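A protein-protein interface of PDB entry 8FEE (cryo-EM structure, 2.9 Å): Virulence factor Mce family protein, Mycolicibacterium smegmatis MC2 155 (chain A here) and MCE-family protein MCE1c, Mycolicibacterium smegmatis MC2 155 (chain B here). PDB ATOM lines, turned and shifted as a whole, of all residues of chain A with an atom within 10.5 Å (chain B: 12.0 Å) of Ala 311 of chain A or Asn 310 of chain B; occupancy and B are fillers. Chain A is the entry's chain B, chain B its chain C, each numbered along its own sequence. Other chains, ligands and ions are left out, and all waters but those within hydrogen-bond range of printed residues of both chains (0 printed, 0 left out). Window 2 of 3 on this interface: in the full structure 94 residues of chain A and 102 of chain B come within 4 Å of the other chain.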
ATOM      1  N   ASN A 308     -11.103  29.211 -17.833  1.00  0.00           N
ATOM      2  CA  ASN A 308     -12.327  28.557 -18.287  1.00  0.00           C
ATOM      3  C   ASN A 308     -11.966  27.640 -19.444  1.00  0.00           C
ATOM      4  O   ASN A 308     -11.710  28.112 -20.554  1.00  0.00           O
ATOM      5  CB  ASN A 308     -13.382  29.577 -18.704  1.00  0.00           C
ATOM      6  CG  ASN A 308     -13.897  30.390 -17.539  1.00  0.00           C
ATOM      7  OD1 ASN A 308     -14.761  29.937 -16.788  1.00  0.00           O
ATOM      8  ND2 ASN A 308     -13.373  31.599 -17.381  1.00  0.00           N
ATOM      9  N   PHE A 309     -11.944  26.337 -19.186  1.00  0.00           N
ATOM     10  CA  PHE A 309     -11.644  25.342 -20.203  1.00  0.00           C
ATOM     11  C   PHE A 309     -12.903  24.556 -20.541  1.00  0.00           C
ATOM     12  O   PHE A 309     -13.703  24.233 -19.658  1.00  0.00           O
ATOM     13  CB  PHE A 309     -10.543  24.387 -19.735  1.00  0.00           C
ATOM     14  CG  PHE A 309      -9.155  24.846 -20.073  1.00  0.00           C
ATOM     15  CD1 PHE A 309      -8.926  26.129 -20.534  1.00  0.00           C
ATOM     16  CD2 PHE A 309      -8.078  23.988 -19.939  1.00  0.00           C
ATOM     17  CE1 PHE A 309      -7.647  26.549 -20.849  1.00  0.00           C
ATOM     18  CE2 PHE A 309      -6.799  24.403 -20.252  1.00  0.00           C
ATOM     19  CZ  PHE A 309      -6.585  25.684 -20.707  1.00  0.00           C
ATOM     20  N   TYR A 310     -13.076  24.260 -21.826  1.00  0.00           N
ATOM     21  CA  TYR A 310     -14.174  23.435 -22.310  1.00  0.00           C
ATOM     22  C   TYR A 310     -13.579  22.281 -23.101  1.00  0.00           C
ATOM     23  O   TYR A 310     -12.812  22.503 -24.044  1.00  0.00           O
ATOM     24  CB  TYR A 310     -15.142  24.249 -23.168  1.00  0.00           C
ATOM     25  CG  TYR A 310     -16.501  23.609 -23.330  1.00  0.00           C
ATOM     26  CD1 TYR A 310     -17.513  23.847 -22.411  1.00  0.00           C
ATOM     27  CD2 TYR A 310     -16.774  22.769 -24.399  1.00  0.00           C
ATOM     28  CE1 TYR A 310     -18.758  23.266 -22.552  1.00  0.00           C
ATOM     29  CE2 TYR A 310     -18.016  22.183 -24.549  1.00  0.00           C
ATOM     30  CZ  TYR A 310     -19.004  22.435 -23.623  1.00  0.00           C
ATOM     31  OH  TYR A 310     -20.242  21.853 -23.768  1.00  0.00           O
ATOM     32  N   ALA A 311     -13.920  21.056 -22.713  1.00  0.00           N
ATOM     33  CA  ALA A 311     -13.409  19.854 -23.368  1.00  0.00           C
ATOM     34  C   ALA A 311     -14.513  19.287 -24.253  1.00  0.00           C
ATOM     35  O   ALA A 311     -15.311  18.453 -23.824  1.00  0.00           O
ATOM     36  CB  ALA A 311     -12.931  18.837 -22.339  1.00  0.00           C
ATOM     37  N   CYS A 312     -14.566  19.762 -25.500  1.00  0.00           N
ATOM     38  CA  CYS A 312     -15.544  19.236 -26.447  1.00  0.00           C
ATOM     39  C   CYS A 312     -15.259  17.776 -26.772  1.00  0.00           C
ATOM     40  O   CYS A 312     -16.151  16.923 -26.687  1.00  0.00           O
ATOM     41  CB  CYS A 312     -15.548  20.076 -27.727  1.00  0.00           C
ATOM     42  SG  CYS A 312     -16.625  21.523 -27.687  1.00  0.00           S
ATOM     43  N   ASP A 313     -14.016  17.467 -27.136  1.00  0.00           N
ATOM     44  CA  ASP A 313     -13.621  16.127 -27.545  1.00  0.00           C
ATOM     45  C   ASP A 313     -12.411  15.698 -26.732  1.00  0.00           C
ATOM     46  O   ASP A 313     -11.443  16.455 -26.611  1.00  0.00           O
ATOM     47  CB  ASP A 313     -13.301  16.082 -29.043  1.00  0.00           C
ATOM     48  CG  ASP A 313     -12.337  17.170 -29.466  1.00  0.00           C
ATOM     49  OD1 ASP A 313     -12.342  18.247 -28.832  1.00  0.00           O
ATOM     50  OD2 ASP A 313     -11.573  16.950 -30.428  1.00  0.00           O
ATOM     51  N   LEU A 314     -12.465  14.491 -26.172  1.00  0.00           N
ATOM     52  CA  LEU A 314     -11.371  13.968 -25.367  1.00  0.00           C
ATOM     53  C   LEU A 314     -11.017  12.562 -25.828  1.00  0.00           C
ATOM     54  O   LEU A 314     -11.898  11.776 -26.189  1.00  0.00           O
ATOM     55  CB  LEU A 314     -11.726  13.972 -23.870  1.00  0.00           C
ATOM     56  CG  LEU A 314     -12.929  13.162 -23.387  1.00  0.00           C
ATOM     57  CD1 LEU A 314     -12.472  11.870 -22.733  1.00  0.00           C
ATOM     58  CD2 LEU A 314     -13.770  13.982 -22.425  1.00  0.00           C
ATOM     59  N   THR A 315      -9.723  12.255 -25.818  1.00  0.00           N
ATOM     60  CA  THR A 315      -9.222  10.952 -26.226  1.00  0.00           C
ATOM     61  C   THR A 315      -8.226  10.446 -25.193  1.00  0.00           C
ATOM     62  O   THR A 315      -7.612  11.222 -24.457  1.00  0.00           O
ATOM     63  CB  THR A 315      -8.555  11.004 -27.609  1.00  0.00           C
ATOM     64  OG1 THR A 315      -7.871   9.771 -27.859  1.00  0.00           O
ATOM     65  CG2 THR A 315      -7.559  12.148 -27.678  1.00  0.00           C
ATOM     66  N   ILE A 332     -13.523   8.626 -25.982  1.00  0.00           N
ATOM     67  CA  ILE A 332     -14.714   8.501 -25.149  1.00  0.00           C
ATOM     68  C   ILE A 332     -15.829   9.368 -25.718  1.00  0.00           C
ATOM     69  O   ILE A 332     -16.904   8.864 -26.064  1.00  0.00           O
ATOM     70  CB  ILE A 332     -14.427   8.873 -23.683  1.00  0.00           C
ATOM     71  CG1 ILE A 332     -13.383   7.931 -23.086  1.00  0.00           C
ATOM     72  CG2 ILE A 332     -15.711   8.842 -22.869  1.00  0.00           C
ATOM     73  CD1 ILE A 332     -13.195   8.098 -21.594  1.00  0.00           C
ATOM     74  N   THR A 333     -15.588  10.676 -25.816  1.00  0.00           N
ATOM     75  CA  THR A 333     -16.584  11.603 -26.336  1.00  0.00           C
ATOM     76  C   THR A 333     -15.939  12.584 -27.304  1.00  0.00           C
ATOM     77  O   THR A 333     -14.802  13.020 -27.102  1.00  0.00           O
ATOM     78  CB  THR A 333     -17.279  12.393 -25.213  1.00  0.00           C
ATOM     79  OG1 THR A 333     -16.299  13.084 -24.429  1.00  0.00           O
ATOM     80  CG2 THR A 333     -18.100  11.474 -24.316  1.00  0.00           C
ATOM     81  N   THR A 334     -16.686  12.926 -28.353  1.00  0.00           N
ATOM     82  CA  THR A 334     -16.342  13.992 -29.282  1.00  0.00           C
ATOM     83  C   THR A 334     -17.602  14.788 -29.586  1.00  0.00           C
ATOM     84  O   THR A 334     -18.722  14.291 -29.437  1.00  0.00           O
ATOM     85  CB  THR A 334     -15.737  13.468 -30.596  1.00  0.00           C
ATOM     86  OG1 THR A 334     -16.639  12.537 -31.206  1.00  0.00           O
ATOM     87  CG2 THR A 334     -14.391  12.802 -30.360  1.00  0.00           C
ATOM     88  N   GLN A 335     -17.412  16.033 -30.012  1.00  0.00           N
ATOM     89  CA  GLN A 335     -18.526  16.899 -30.399  1.00  0.00           C
ATOM     90  C   GLN A 335     -18.385  17.295 -31.861  1.00  0.00           C
ATOM     91  O   GLN A 335     -17.546  18.149 -32.199  1.00  0.00           O
ATOM     92  CB  GLN A 335     -18.593  18.138 -29.509  1.00  0.00           C
ATOM     93  CG  GLN A 335     -19.952  18.821 -29.522  1.00  0.00           C
ATOM     94  CD  GLN A 335     -20.114  19.830 -28.403  1.00  0.00           C
ATOM     95  OE1 GLN A 335     -21.232  20.157 -28.001  1.00  0.00           O
ATOM     96  NE2 GLN A 335     -18.997  20.328 -27.889  1.00  0.00           N
ATOM     97  N   PRO A 336     -19.169  16.698 -32.763  1.00  0.00           N
ATOM     98  CA  PRO A 336     -19.043  17.055 -34.184  1.00  0.00           C
ATOM     99  C   PRO A 336     -19.584  18.436 -34.498  1.00  0.00           C
ATOM    100  O   PRO A 336     -18.937  19.198 -35.228  1.00  0.00           O
ATOM    101  CB  PRO A 336     -19.841  15.953 -34.899  1.00  0.00           C
ATOM    102  CG  PRO A 336     -20.056  14.876 -33.868  1.00  0.00           C
ATOM    103  CD  PRO A 336     -20.109  15.586 -32.556  1.00  0.00           C
ATOM    104  N   ARG A 339     -21.091  24.434 -30.464  1.00  0.00           N
ATOM    105  CA  ARG A 339     -20.219  25.566 -30.171  1.00  0.00           C
ATOM    106  C   ARG A 339     -18.787  25.362 -30.658  1.00  0.00           C
ATOM    107  O   ARG A 339     -18.054  26.344 -30.808  1.00  0.00           O
ATOM    108  CB  ARG A 339     -20.213  25.852 -28.669  1.00  0.00           C
ATOM    109  CG  ARG A 339     -19.935  24.636 -27.812  1.00  0.00           C
ATOM    110  CD  ARG A 339     -19.359  25.024 -26.460  1.00  0.00           C
ATOM    111  NE  ARG A 339     -18.032  25.617 -26.570  1.00  0.00           N
ATOM    112  CZ  ARG A 339     -17.679  26.773 -26.025  1.00  0.00           C
ATOM    113  NH1 ARG A 339     -18.528  27.485 -25.304  1.00  0.00           N
ATOM    114  NH2 ARG A 339     -16.439  27.220 -26.199  1.00  0.00           N
ATOM    115  N   CYS A 340     -18.374  24.121 -30.903  1.00  0.00           N
ATOM    116  CA  CYS A 340     -17.035  23.796 -31.396  1.00  0.00           C
ATOM    117  C   CYS A 340     -17.152  23.131 -32.764  1.00  0.00           C
ATOM    118  O   CYS A 340     -17.173  21.904 -32.879  1.00  0.00           O
ATOM    119  CB  CYS A 340     -16.300  22.904 -30.380  1.00  0.00           C
ATOM    120  SG  CYS A 340     -17.356  21.675 -29.579  1.00  0.00           S
ATOM    121  N   VAL B 306      -7.656  25.764 -13.672  1.00  0.00           N
ATOM    122  CA  VAL B 306      -8.560  25.597 -14.802  1.00  0.00           C
ATOM    123  C   VAL B 306      -9.892  25.081 -14.283  1.00  0.00           C
ATOM    124  O   VAL B 306      -9.954  24.347 -13.293  1.00  0.00           O
ATOM    125  CB  VAL B 306      -7.998  24.638 -15.873  1.00  0.00           C
ATOM    126  CG1 VAL B 306      -6.858  25.281 -16.620  1.00  0.00           C
ATOM    127  CG2 VAL B 306      -7.539  23.340 -15.233  1.00  0.00           C
ATOM    128  N   MET B 307     -10.966  25.484 -14.951  1.00  0.00           N
ATOM    129  CA  MET B 307     -12.301  24.973 -14.675  1.00  0.00           C
ATOM    130  C   MET B 307     -12.738  24.123 -15.859  1.00  0.00           C
ATOM    131  O   MET B 307     -12.775  24.609 -16.994  1.00  0.00           O
ATOM    132  CB  MET B 307     -13.297  26.104 -14.425  1.00  0.00           C
ATOM    133  CG  MET B 307     -14.657  25.605 -13.972  1.00  0.00           C
ATOM    134  SD  MET B 307     -15.860  26.914 -13.690  1.00  0.00           S
ATOM    135  CE  MET B 307     -17.230  25.960 -13.046  1.00  0.00           C
ATOM    136  N   LEU B 308     -13.063  22.864 -15.596  1.00  0.00           N
ATOM    137  CA  LEU B 308     -13.508  21.930 -16.625  1.00  0.00           C
ATOM    138  C   LEU B 308     -14.998  21.688 -16.416  1.00  0.00           C
ATOM    139  O   LEU B 308     -15.398  20.968 -15.497  1.00  0.00           O
ATOM    140  CB  LEU B 308     -12.708  20.633 -16.559  1.00  0.00           C
ATOM    141  CG  LEU B 308     -11.195  20.773 -16.728  1.00  0.00           C
ATOM    142  CD1 LEU B 308     -10.481  19.518 -16.257  1.00  0.00           C
ATOM    143  CD2 LEU B 308     -10.852  21.070 -18.174  1.00  0.00           C
ATOM    144  N   VAL B 309     -15.820  22.301 -17.275  1.00  0.00           N
ATOM    145  CA  VAL B 309     -17.272  22.171 -17.173  1.00  0.00           C
ATOM    146  C   VAL B 309     -17.765  20.871 -17.793  1.00  0.00           C
ATOM    147  O   VAL B 309     -18.943  20.519 -17.648  1.00  0.00           O
ATOM    148  CB  VAL B 309     -17.860  23.459 -17.796  1.00  0.00           C
ATOM    149  CG1 VAL B 309     -19.389  23.453 -17.877  1.00  0.00           C
ATOM    150  CG2 VAL B 309     -17.374  24.682 -17.034  1.00  0.00           C
ATOM    151  N   ASN B 310     -16.875  20.094 -18.399  1.00  0.00           N
ATOM    152  CA  ASN B 310     -17.237  18.785 -18.929  1.00  0.00           C
ATOM    153  C   ASN B 310     -16.784  17.670 -17.992  1.00  0.00           C
ATOM    154  O   ASN B 310     -15.609  17.301 -17.970  1.00  0.00           O
ATOM    155  CB  ASN B 310     -16.630  18.587 -20.316  1.00  0.00           C
ATOM    156  CG  ASN B 310     -17.140  19.596 -21.321  1.00  0.00           C
ATOM    157  OD1 ASN B 310     -16.400  20.471 -21.767  1.00  0.00           O
ATOM    158  ND2 ASN B 310     -18.410  19.478 -21.685  1.00  0.00           N
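O of Met 307 of chain B is in hydrogen-bond range of N of Phe 309 of chain A (2.9 Å).
OD1 of Asn 310 of chain B sits at hydrogen-bond distance from N of Ala 311 of chain A.
Printed residues of chain B within 4 Å of Ala 311 of chain A: Asn 310.
Asn 310 of chain B touches two residues of chain A.
Tyr 310 of chain A touches just one residue of chain B: Asn 310 (3.5 Å).
No residue of chain B comes within 4 Å of Cys 312 of chain A.
Of the printed residues of chain A, Leu 308 of chain B touches Phe 309 (3.7 Å).
Of the printed residues of chain A, Val 306 of chain B touches Phe 309.
Of the printed residues of chain A, Met 307 of chain B touches Asn 308 and Phe 309.
Of the printed residues of chain B, Phe 309 of chain A touches Val 306 (3.7 Å), Met 307 (2.8 Å), Leu 308 (3.7 Å) and Val 309 (3.7 Å).
Thr 315 of chain A touches none of the printed residues of chain B.
The nearest residue of chain A that does not touch Asn 310 of chain B is Cys 312 of chain A (4.2 Å).
Met 307 of chain B touches Asn 308 of chain A (O to C, 3.98 Å).
Val 306 of chain B touches Phe 309 of chain A (CG1 to CE2, 3.7 Å).
CB of Phe 309 of chain A touches CD2 of Leu 308 of chain B, at 3.7 Å.
N of Val 309 of chain B touches O of Phe 309 of chain A (3.7 Å).
Tyr 310 of chain A touches Asn 310 of chain B (CG to OD1, 3.5 Å).
The side-chain sulfur (SG) of Cys 340 of chain A forms a disulfide with the side-chain sulfur (SG) of Cys 312 of chain A, 2.0 Å away.
Of the 15 printed residues of chain A, 4 touch a printed residue of chain B.
Hydrophobic or aromatic side chains of chain A that line the printed part of chain B: Phe 309, Tyr 310 and Ala 311.
Among the printed residues, no Asp or Glu carboxylate lies within 4 Å of a Lys or Arg side-chain nitrogen of the other chain.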
